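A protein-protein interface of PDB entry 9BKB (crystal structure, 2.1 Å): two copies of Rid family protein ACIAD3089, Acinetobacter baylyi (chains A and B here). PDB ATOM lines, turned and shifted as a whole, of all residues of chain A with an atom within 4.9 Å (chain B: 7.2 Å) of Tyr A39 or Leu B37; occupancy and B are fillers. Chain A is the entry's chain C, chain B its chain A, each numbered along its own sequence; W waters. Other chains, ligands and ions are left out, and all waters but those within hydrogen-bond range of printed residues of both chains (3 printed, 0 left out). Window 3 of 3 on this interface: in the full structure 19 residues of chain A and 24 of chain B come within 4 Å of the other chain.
Printed residues of chain B within 4 Å of Ile A32: Leu B95 (3.9 Å) and Thr B133 (3.6 Å).
Tyr A39 touches just these residues of chain B: Leu B37 (3.6 Å), Leu B95 (3.6 Å) and Thr B133 (3.4 Å).
Printed residues of chain A within 4 Å of Leu B37: His A34 and Tyr A39.
Tyr B39 touches none of the printed residues of chain A.
Of the printed residues of chain A, Ala B155 touches His A34 (3.7 Å).
Gln B158 touches none of the printed residues of chain A.
The nearest printed residue of chain B that does not touch Tyr A39 is Ile B153 (4.6 Å).
The nearest printed residue of chain A that does not touch Leu B37 is Leu A37 (6.2 Å).
The nearest printed residue of chain B that does not touch His A34 is Gly B36 (4.8 Å).
Water W2 lies within hydrogen-bond range of O of Met A40, OG1 of Thr B133 and NE2 of Gln B96.
Water W3 lies within hydrogen-bond range of the backbone carbonyl oxygen (O) of Leu B156 (2.8 Å), a ring nitrogen (NE2) of His A34 (3.0 Å) and the backbone carbonyl oxygen (O) of Gly B36 (3.1 Å).
Water W1 lies within hydrogen-bond range of OH of Tyr A39 and OH of Tyr B39.
Of the 11 printed residues of chain A, 5 touch a printed residue of chain B.
Along chain A the printed residues that touch a printed residue of chain B span positions 31 to 41.
Among the printed residues, no Asp or Glu carboxylate lies within 4 Å of a Lys or Arg side-chain nitrogen of the other chain.
His A34 touches Leu B37, but with the chains exchanged Leu A37 does not touch His B34 (9.9 Å).
Tyr A39 touches Leu B37, but with the chains exchanged Leu A37 does not touch Tyr B39 (7.0 Å).
Among the printed residues, pairs that only touch across the chains: Ser A41 with Thr B133, Tyr A39 with Thr B133, Ile A32 with Thr B133, Tyr A39 with Leu B95, Tyr A39 with Leu B37, His A34 with Leu B37, His A34 with Ala B155, His A34 with Leu B95, Leu A31 with Thr B133 and Ile A32 with Leu B95.
The backbone NH of Arg B134 lies within hydrogen-bond range of the side-chain hydroxyl of Ser A41, at 2.9 Å.
The backbone carbonyl oxygen (O) of Ile A32 is in hydrogen-bond range of the backbone NH (N) of Tyr A39 (2.9 Å).
The backbone NH of Leu B95 sits at hydrogen-bond distance from the backbone carbonyl oxygen of Ile B153 (2.7 Å).
The backbone NH of Ala B155 lies within hydrogen-bond range of the backbone carbonyl oxygen of Lys B93 (2.7 Å).
N of Ser A41 is in hydrogen-bond range of O of Ser A30, 2.9 Å away.
O of Leu B95 lies within hydrogen-bond range of OG1 of Thr B133 (2.7 Å).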
ATOM      1  N   SER A  30      37.510 -23.910 -27.501  1.00  0.00           N
ATOM      2  CA  SER A  30      38.555 -22.894 -27.392  1.00  0.00           C
ATOM      3  C   SER A  30      38.009 -21.492 -27.635  1.00  0.00           C
ATOM      4  O   SER A  30      38.441 -20.527 -26.984  1.00  0.00           O
ATOM      5  CB  SER A  30      39.682 -23.186 -28.389  1.00  0.00           C
ATOM      6  OG  SER A  30      40.456 -24.300 -27.957  1.00  0.00           O
ATOM      7  N   LEU A  31      37.072 -21.354 -28.567  1.00  0.00           N
ATOM      8  CA  LEU A  31      36.595 -20.048 -28.999  1.00  0.00           C
ATOM      9  C   LEU A  31      35.132 -20.173 -29.378  1.00  0.00           C
ATOM     10  O   LEU A  31      34.737 -21.119 -30.067  1.00  0.00           O
ATOM     11  CB  LEU A  31      37.419 -19.523 -30.191  1.00  0.00           C
ATOM     12  CG  LEU A  31      37.010 -18.197 -30.856  1.00  0.00           C
ATOM     13  CD1 LEU A  31      38.212 -17.532 -31.522  1.00  0.00           C
ATOM     14  CD2 LEU A  31      35.865 -18.359 -31.879  1.00  0.00           C
ATOM     15  N   ILE A  32      34.329 -19.208 -28.948  1.00  0.00           N
ATOM     16  CA  ILE A  32      32.932 -19.135 -29.368  1.00  0.00           C
ATOM     17  C   ILE A  32      32.644 -17.715 -29.822  1.00  0.00           C
ATOM     18  O   ILE A  32      32.997 -16.761 -29.123  1.00  0.00           O
ATOM     19  CB  ILE A  32      31.972 -19.545 -28.237  1.00  0.00           C
ATOM     20  CG1 ILE A  32      32.148 -21.028 -27.917  1.00  0.00           C
ATOM     21  CG2 ILE A  32      30.511 -19.266 -28.630  1.00  0.00           C
ATOM     22  CD1 ILE A  32      31.188 -21.516 -26.863  1.00  0.00           C
ATOM     23  N   HIS A  34      29.867 -14.756 -30.787  1.00  0.00           N
ATOM     24  CA  HIS A  34      28.491 -14.307 -30.629  1.00  0.00           C
ATOM     25  C   HIS A  34      28.444 -12.802 -30.817  1.00  0.00           C
ATOM     26  O   HIS A  34      29.206 -12.070 -30.172  1.00  0.00           O
ATOM     27  CB  HIS A  34      27.921 -14.674 -29.258  1.00  0.00           C
ATOM     28  CG  HIS A  34      26.473 -14.324 -29.106  1.00  0.00           C
ATOM     29  ND1 HIS A  34      26.049 -13.123 -28.575  1.00  0.00           N
ATOM     30  CD2 HIS A  34      25.353 -15.011 -29.424  1.00  0.00           C
ATOM     31  CE1 HIS A  34      24.730 -13.087 -28.569  1.00  0.00           C
ATOM     32  NE2 HIS A  34      24.282 -14.222 -29.073  1.00  0.00           N
ATOM     33  N   LEU A  37      31.610 -10.828 -31.352  1.00  0.00           N
ATOM     34  CA  LEU A  37      32.693 -11.012 -30.387  1.00  0.00           C
ATOM     35  C   LEU A  37      33.132 -12.469 -30.347  1.00  0.00           C
ATOM     36  O   LEU A  37      32.302 -13.374 -30.375  1.00  0.00           O
ATOM     37  CB  LEU A  37      32.295 -10.583 -28.954  1.00  0.00           C
ATOM     38  CG  LEU A  37      32.252  -9.089 -28.567  1.00  0.00           C
ATOM     39  CD1 LEU A  37      31.685  -8.205 -29.627  1.00  0.00           C
ATOM     40  CD2 LEU A  37      31.531  -8.879 -27.236  1.00  0.00           C
ATOM     41  N   ALA A  38      34.432 -12.690 -30.225  1.00  0.00           N
ATOM     42  CA  ALA A  38      34.990 -14.011 -29.980  1.00  0.00           C
ATOM     43  C   ALA A  38      35.420 -14.097 -28.514  1.00  0.00           C
ATOM     44  O   ALA A  38      36.310 -13.359 -28.075  1.00  0.00           O
ATOM     45  CB  ALA A  38      36.172 -14.289 -30.902  1.00  0.00           C
ATOM     46  N   TYR A  39      34.768 -14.980 -27.769  1.00  0.00           N
ATOM     47  CA  TYR A  39      35.151 -15.333 -26.410  1.00  0.00           C
ATOM     48  C   TYR A  39      36.155 -16.477 -26.479  1.00  0.00           C
ATOM     49  O   TYR A  39      35.938 -17.455 -27.202  1.00  0.00           O
ATOM     50  CB  TYR A  39      33.913 -15.748 -25.617  1.00  0.00           C
ATOM     51  CG  TYR A  39      32.855 -14.667 -25.521  1.00  0.00           C
ATOM     52  CD1 TYR A  39      31.999 -14.395 -26.590  1.00  0.00           C
ATOM     53  CD2 TYR A  39      32.717 -13.907 -24.364  1.00  0.00           C
ATOM     54  CE1 TYR A  39      31.030 -13.390 -26.498  1.00  0.00           C
ATOM     55  CE2 TYR A  39      31.771 -12.923 -24.265  1.00  0.00           C
ATOM     56  CZ  TYR A  39      30.926 -12.658 -25.330  1.00  0.00           C
ATOM     57  OH  TYR A  39      29.974 -11.656 -25.214  1.00  0.00           O
ATOM     58  N   MET A  40      37.256 -16.364 -25.743  1.00  0.00           N
ATOM     59  CA  MET A  40      38.297 -17.377 -25.800  1.00  0.00           C
ATOM     60  C   MET A  40      38.558 -17.957 -24.421  1.00  0.00           C
ATOM     61  O   MET A  40      38.620 -17.223 -23.421  1.00  0.00           O
ATOM     62  CB  MET A  40      39.587 -16.803 -26.381  1.00  0.00           C
ATOM     63  CG  MET A  40      39.375 -16.016 -27.686  1.00  0.00           C
ATOM     64  SD  MET A  40      40.898 -15.702 -28.619  1.00  0.00           S
ATOM     65  CE  MET A  40      41.537 -17.365 -28.819  1.00  0.00           C
ATOM     66  N   SER A  41      38.724 -19.276 -24.390  1.00  0.00           N
ATOM     67  CA  SER A  41      39.066 -19.996 -23.174  1.00  0.00           C
ATOM     68  C   SER A  41      40.443 -19.574 -22.664  1.00  0.00           C
ATOM     69  O   SER A  41      41.265 -19.046 -23.401  1.00  0.00           O
ATOM     70  CB  SER A  41      39.054 -21.502 -23.439  1.00  0.00           C
ATOM     71  OG  SER A  41      37.731 -21.949 -23.684  1.00  0.00           O
ATOM     72  N   PHE A 152      40.669 -14.163 -23.141  1.00  0.00           N
ATOM     73  CA  PHE A 152      40.473 -12.995 -23.992  1.00  0.00           C
ATOM     74  C   PHE A 152      39.021 -12.866 -24.427  1.00  0.00           C
ATOM     75  O   PHE A 152      38.320 -13.864 -24.629  1.00  0.00           O
ATOM     76  CB  PHE A 152      41.316 -13.025 -25.278  1.00  0.00           C
ATOM     77  CG  PHE A 152      42.804 -13.131 -25.067  1.00  0.00           C
ATOM     78  CD1 PHE A 152      43.404 -14.361 -24.836  1.00  0.00           C
ATOM     79  CD2 PHE A 152      43.605 -12.015 -25.188  1.00  0.00           C
ATOM     80  CE1 PHE A 152      44.764 -14.457 -24.670  1.00  0.00           C
ATOM     81  CE2 PHE A 152      44.975 -12.105 -25.027  1.00  0.00           C
ATOM     82  CZ  PHE A 152      45.557 -13.322 -24.776  1.00  0.00           C
ATOM     83  N   ILE A 153      38.594 -11.616 -24.612  1.00  0.00           N
ATOM     84  CA  ILE A 153      37.421 -11.272 -25.416  1.00  0.00           C
ATOM     85  C   ILE A 153      37.868 -10.326 -26.524  1.00  0.00           C
ATOM     86  O   ILE A 153      38.501  -9.292 -26.248  1.00  0.00           O
ATOM     87  CB  ILE A 153      36.297 -10.647 -24.573  1.00  0.00           C
ATOM     88  CG1 ILE A 153      35.908 -11.581 -23.446  1.00  0.00           C
ATOM     89  CG2 ILE A 153      35.074 -10.393 -25.434  1.00  0.00           C
ATOM     90  CD1 ILE A 153      34.772 -11.030 -22.566  1.00  0.00           C
ATOM     91  N   LEU B  31      21.346 -12.531 -11.586  1.00  0.00           N
ATOM     92  CA  LEU B  31      21.365 -12.562 -13.038  1.00  0.00           C
ATOM     93  C   LEU B  31      20.897 -11.219 -13.554  1.00  0.00           C
ATOM     94  O   LEU B  31      19.913 -10.672 -13.063  1.00  0.00           O
ATOM     95  CB  LEU B  31      20.469 -13.697 -13.560  1.00  0.00           C
ATOM     96  CG  LEU B  31      20.322 -13.877 -15.074  1.00  0.00           C
ATOM     97  CD1 LEU B  31      20.004 -15.338 -15.339  1.00  0.00           C
ATOM     98  CD2 LEU B  31      19.227 -12.990 -15.660  1.00  0.00           C
ATOM     99  N   ILE B  32      21.595 -10.690 -14.553  1.00  0.00           N
ATOM    100  CA  ILE B  32      21.137  -9.490 -15.237  1.00  0.00           C
ATOM    101  C   ILE B  32      21.189  -9.734 -16.734  1.00  0.00           C
ATOM    102  O   ILE B  32      22.208 -10.198 -17.255  1.00  0.00           O
ATOM    103  CB  ILE B  32      21.968  -8.246 -14.863  1.00  0.00           C
ATOM    104  CG1 ILE B  32      21.695  -7.841 -13.417  1.00  0.00           C
ATOM    105  CG2 ILE B  32      21.672  -7.093 -15.817  1.00  0.00           C
ATOM    106  CD1 ILE B  32      22.405  -6.576 -13.002  1.00  0.00           C
ATOM    107  N   GLU B  33      20.108  -9.383 -17.433  1.00  0.00           N
ATOM    108  CA  GLU B  33      20.057  -9.527 -18.879  1.00  0.00           C
ATOM    109  C   GLU B  33      20.338  -8.200 -19.578  1.00  0.00           C
ATOM    110  O   GLU B  33      19.803  -7.153 -19.202  1.00  0.00           O
ATOM    111  CB  GLU B  33      18.698 -10.063 -19.322  1.00  0.00           C
ATOM    112  CG  GLU B  33      18.530 -10.018 -20.819  1.00  0.00           C
ATOM    113  CD  GLU B  33      17.189 -10.539 -21.277  1.00  0.00           C
ATOM    114  OE1 GLU B  33      16.470 -11.152 -20.464  1.00  0.00           O
ATOM    115  OE2 GLU B  33      16.853 -10.297 -22.453  1.00  0.00           O
ATOM    116  N   HIS B  34      21.166  -8.251 -20.610  1.00  0.00           N
ATOM    117  CA  HIS B  34      21.404  -7.085 -21.443  1.00  0.00           C
ATOM    118  C   HIS B  34      21.754  -7.534 -22.852  1.00  0.00           C
ATOM    119  O   HIS B  34      22.626  -8.390 -23.039  1.00  0.00           O
ATOM    120  CB  HIS B  34      22.518  -6.197 -20.875  1.00  0.00           C
ATOM    121  CG  HIS B  34      22.708  -4.932 -21.647  1.00  0.00           C
ATOM    122  ND1 HIS B  34      23.644  -4.809 -22.649  1.00  0.00           N
ATOM    123  CD2 HIS B  34      22.046  -3.753 -21.601  1.00  0.00           C
ATOM    124  CE1 HIS B  34      23.572  -3.597 -23.167  1.00  0.00           C
ATOM    125  NE2 HIS B  34      22.606  -2.939 -22.554  1.00  0.00           N
ATOM    126  N   ALA B  35      21.052  -6.965 -23.833  1.00  0.00           N
ATOM    127  CA  ALA B  35      21.318  -7.195 -25.254  1.00  0.00           C
ATOM    128  C   ALA B  35      21.362  -8.685 -25.588  1.00  0.00           C
ATOM    129  O   ALA B  35      22.226  -9.154 -26.327  1.00  0.00           O
ATOM    130  CB  ALA B  35      22.614  -6.507 -25.686  1.00  0.00           C
ATOM    131  N   GLY B  36      20.419  -9.443 -25.046  1.00  0.00           N
ATOM    132  CA  GLY B  36      20.379 -10.861 -25.352  1.00  0.00           C
ATOM    133  C   GLY B  36      21.393 -11.726 -24.629  1.00  0.00           C
ATOM    134  O   GLY B  36      21.502 -12.913 -24.957  1.00  0.00           O
ATOM    135  N   LEU B  37      22.122 -11.188 -23.645  1.00  0.00           N
ATOM    136  CA  LEU B  37      23.060 -11.960 -22.834  1.00  0.00           C
ATOM    137  C   LEU B  37      22.592 -11.939 -21.387  1.00  0.00           C
ATOM    138  O   LEU B  37      22.100 -10.919 -20.907  1.00  0.00           O
ATOM    139  CB  LEU B  37      24.471 -11.369 -22.907  1.00  0.00           C
ATOM    140  CG  LEU B  37      25.181 -11.404 -24.265  1.00  0.00           C
ATOM    141  CD1 LEU B  37      26.617 -10.948 -24.124  1.00  0.00           C
ATOM    142  CD2 LEU B  37      25.103 -12.772 -24.940  1.00  0.00           C
ATOM    143  N   ALA B  38      22.721 -13.059 -20.685  1.00  0.00           N
ATOM    144  CA  ALA B  38      22.485 -13.106 -19.247  1.00  0.00           C
ATOM    145  C   ALA B  38      23.834 -13.231 -18.548  1.00  0.00           C
ATOM    146  O   ALA B  38      24.553 -14.213 -18.753  1.00  0.00           O
ATOM    147  CB  ALA B  38      21.558 -14.263 -18.870  1.00  0.00           C
ATOM    148  N   TYR B  39      24.186 -12.219 -17.758  1.00  0.00           N
ATOM    149  CA  TYR B  39      25.351 -12.256 -16.882  1.00  0.00           C
ATOM    150  C   TYR B  39      24.928 -12.858 -15.554  1.00  0.00           C
ATOM    151  O   TYR B  39      23.887 -12.477 -15.007  1.00  0.00           O
ATOM    152  CB  TYR B  39      25.905 -10.843 -16.675  1.00  0.00           C
ATOM    153  CG  TYR B  39      26.330 -10.213 -17.976  1.00  0.00           C
ATOM    154  CD1 TYR B  39      25.390  -9.675 -18.850  1.00  0.00           C
ATOM    155  CD2 TYR B  39      27.664 -10.183 -18.352  1.00  0.00           C
ATOM    156  CE1 TYR B  39      25.770  -9.123 -20.049  1.00  0.00           C
ATOM    157  CE2 TYR B  39      28.052  -9.626 -19.548  1.00  0.00           C
ATOM    158  CZ  TYR B  39      27.101  -9.094 -20.390  1.00  0.00           C
ATOM    159  OH  TYR B  39      27.483  -8.545 -21.593  1.00  0.00           O
ATOM    160  N   TYR B  85      13.383 -17.286 -16.422  1.00  0.00           N
ATOM    161  CA  TYR B  85      12.784 -17.363 -17.748  1.00  0.00           C
ATOM    162  C   TYR B  85      11.721 -18.443 -17.876  1.00  0.00           C
ATOM    163  O   TYR B  85      11.111 -18.565 -18.943  1.00  0.00           O
ATOM    164  CB  TYR B  85      13.871 -17.602 -18.812  1.00  0.00           C
ATOM    165  CG  TYR B  85      14.843 -16.460 -18.916  1.00  0.00           C
ATOM    166  CD1 TYR B  85      14.500 -15.298 -19.600  1.00  0.00           C
ATOM    167  CD2 TYR B  85      16.081 -16.514 -18.286  1.00  0.00           C
ATOM    168  CE1 TYR B  85      15.366 -14.230 -19.675  1.00  0.00           C
ATOM    169  CE2 TYR B  85      16.963 -15.442 -18.354  1.00  0.00           C
ATOM    170  CZ  TYR B  85      16.599 -14.304 -19.050  1.00  0.00           C
ATOM    171  OH  TYR B  85      17.465 -13.236 -19.124  1.00  0.00           O
ATOM    172  N   LYS B  93      23.444 -20.475 -26.004  1.00  0.00           N
ATOM    173  CA  LYS B  93      24.830 -20.898 -25.815  1.00  0.00           C
ATOM    174  C   LYS B  93      25.320 -20.406 -24.459  1.00  0.00           C
ATOM    175  O   LYS B  93      24.961 -19.309 -24.041  1.00  0.00           O
ATOM    176  CB  LYS B  93      25.737 -20.346 -26.925  1.00  0.00           C
ATOM    177  CG  LYS B  93      26.991 -21.178 -27.222  1.00  0.00           C
ATOM    178  CD  LYS B  93      26.757 -22.352 -28.162  1.00  0.00           C
ATOM    179  CE  LYS B  93      26.738 -21.929 -29.613  1.00  0.00           C
ATOM    180  NZ  LYS B  93      26.757 -23.145 -30.475  1.00  0.00           N
ATOM    181  N   LEU B  95      28.231 -18.787 -23.245  1.00  0.00           N
ATOM    182  CA  LEU B  95      29.390 -18.188 -23.897  1.00  0.00           C
ATOM    183  C   LEU B  95      30.645 -18.398 -23.068  1.00  0.00           C
ATOM    184  O   LEU B  95      31.720 -18.692 -23.611  1.00  0.00           O
ATOM    185  CB  LEU B  95      29.158 -16.698 -24.145  1.00  0.00           C
ATOM    186  CG  LEU B  95      27.990 -16.344 -25.084  1.00  0.00           C
ATOM    187  CD1 LEU B  95      27.952 -14.841 -25.343  1.00  0.00           C
ATOM    188  CD2 LEU B  95      28.079 -17.118 -26.391  1.00  0.00           C
ATOM    189  N   GLN B  96      30.530 -18.253 -21.751  1.00  0.00           N
ATOM    190  CA  GLN B  96      31.724 -18.290 -20.920  1.00  0.00           C
ATOM    191  C   GLN B  96      31.385 -18.846 -19.545  1.00  0.00           C
ATOM    192  O   GLN B  96      30.335 -18.526 -18.975  1.00  0.00           O
ATOM    193  CB  GLN B  96      32.346 -16.895 -20.797  1.00  0.00           C
ATOM    194  CG  GLN B  96      33.596 -16.823 -19.939  1.00  0.00           C
ATOM    195  CD  GLN B  96      34.045 -15.389 -19.735  1.00  0.00           C
ATOM    196  OE1 GLN B  96      33.506 -14.672 -18.887  1.00  0.00           O
ATOM    197  NE2 GLN B  96      35.028 -14.959 -20.518  1.00  0.00           N
ATOM    198  N   THR B 133      33.078 -21.712 -23.699  1.00  0.00           N
ATOM    199  CA  THR B 133      34.486 -21.479 -23.400  1.00  0.00           C
ATOM    200  C   THR B 133      34.654 -21.534 -21.878  1.00  0.00           C
ATOM    201  O   THR B 133      33.686 -21.420 -21.116  1.00  0.00           O
ATOM    202  CB  THR B 133      34.998 -20.148 -23.975  1.00  0.00           C
ATOM    203  OG1 THR B 133      34.407 -19.045 -23.270  1.00  0.00           O
ATOM    204  CG2 THR B 133      34.665 -20.033 -25.479  1.00  0.00           C
ATOM    205  N   ARG B 134      35.894 -21.722 -21.434  1.00  0.00           N
ATOM    206  CA  ARG B 134      36.103 -21.978 -20.020  1.00  0.00           C
ATOM    207  C   ARG B 134      37.478 -21.500 -19.572  1.00  0.00           C
ATOM    208  O   ARG B 134      38.441 -21.521 -20.338  1.00  0.00           O
ATOM    209  CB  ARG B 134      35.985 -23.494 -19.783  1.00  0.00           C
ATOM    210  CG  ARG B 134      35.832 -23.949 -18.375  1.00  0.00           C
ATOM    211  CD  ARG B 134      35.720 -25.487 -18.363  1.00  0.00           C
ATOM    212  NE  ARG B 134      37.003 -26.176 -18.445  1.00  0.00           N
ATOM    213  CZ  ARG B 134      37.135 -27.498 -18.449  1.00  0.00           C
ATOM    214  NH1 ARG B 134      36.078 -28.298 -18.393  1.00  0.00           N
ATOM    215  NH2 ARG B 134      38.351 -28.030 -18.488  1.00  0.00           N
ATOM    216  N   ILE B 153      28.440 -16.381 -18.437  1.00  0.00           N
ATOM    217  CA  ILE B 153      27.763 -15.521 -19.406  1.00  0.00           C
ATOM    218  C   ILE B 153      27.042 -16.427 -20.397  1.00  0.00           C
ATOM    219  O   ILE B 153      27.684 -17.281 -21.027  1.00  0.00           O
ATOM    220  CB  ILE B 153      28.750 -14.611 -20.160  1.00  0.00           C
ATOM    221  CG1 ILE B 153      29.605 -13.797 -19.174  1.00  0.00           C
ATOM    222  CG2 ILE B 153      27.991 -13.760 -21.211  1.00  0.00           C
ATOM    223  CD1 ILE B 153      30.517 -12.771 -19.857  1.00  0.00           C
ATOM    224  N   VAL B 154      25.729 -16.218 -20.559  1.00  0.00           N
ATOM    225  CA  VAL B 154      24.853 -17.098 -21.333  1.00  0.00           C
ATOM    226  C   VAL B 154      24.150 -16.299 -22.431  1.00  0.00           C
ATOM    227  O   VAL B 154      23.470 -15.310 -22.142  1.00  0.00           O
ATOM    228  CB  VAL B 154      23.812 -17.766 -20.416  1.00  0.00           C
ATOM    229  CG1 VAL B 154      22.967 -18.763 -21.190  1.00  0.00           C
ATOM    230  CG2 VAL B 154      24.504 -18.461 -19.237  1.00  0.00           C
ATOM    231  N   ALA B 155      24.251 -16.754 -23.678  1.00  0.00           N
ATOM    232  CA  ALA B 155      23.464 -16.144 -24.750  1.00  0.00           C
ATOM    233  C   ALA B 155      22.038 -16.700 -24.751  1.00  0.00           C
ATOM    234  O   ALA B 155      21.820 -17.903 -24.571  1.00  0.00           O
ATOM    235  CB  ALA B 155      24.131 -16.366 -26.108  1.00  0.00           C
ATOM    236  N   LEU B 156      21.061 -15.808 -24.924  1.00  0.00           N
ATOM    237  CA  LEU B 156      19.647 -16.164 -24.945  1.00  0.00           C
ATOM    238  C   LEU B 156      19.157 -16.201 -26.392  1.00  0.00           C
ATOM    239  O   LEU B 156      19.664 -15.478 -27.252  1.00  0.00           O
ATOM    240  CB  LEU B 156      18.802 -15.186 -24.122  1.00  0.00           C
ATOM    241  CG  LEU B 156      19.279 -14.987 -22.679  1.00  0.00           C
ATOM    242  CD1 LEU B 156      18.503 -13.860 -22.027  1.00  0.00           C
ATOM    243  CD2 LEU B 156      19.160 -16.256 -21.868  1.00  0.00           C
ATOM    244  N   GLN B 158      16.395 -15.294 -28.155  1.00  0.00           N
ATOM    245  CA  GLN B 158      15.784 -14.178 -28.907  1.00  0.00           C
ATOM    246  C   GLN B 158      14.848 -14.685 -30.005  1.00  0.00           C
ATOM    247  O   GLN B 158      13.641 -14.468 -29.947  1.00  0.00           O
ATOM    248  CB  GLN B 158      16.849 -13.262 -29.541  1.00  0.00           C
ATOM    249  CG  GLN B 158      17.723 -12.554 -28.533  1.00  0.00           C
ATOM    250  CD  GLN B 158      16.929 -11.579 -27.697  1.00  0.00           C
ATOM    251  OE1 GLN B 158      16.675 -11.806 -26.507  1.00  0.00           O
ATOM    252  NE2 GLN B 158      16.518 -10.482 -28.320  1.00  0.00           N
HETATM  253  O   HOH W   1      30.233  -9.280 -23.437  1.00  0.00           O
HETATM  254  O   HOH W   2      36.282 -17.332 -22.031  1.00  0.00           O
HETATM  255  O   HOH W   3      21.599 -13.586 -27.971  1.00  0.00           O
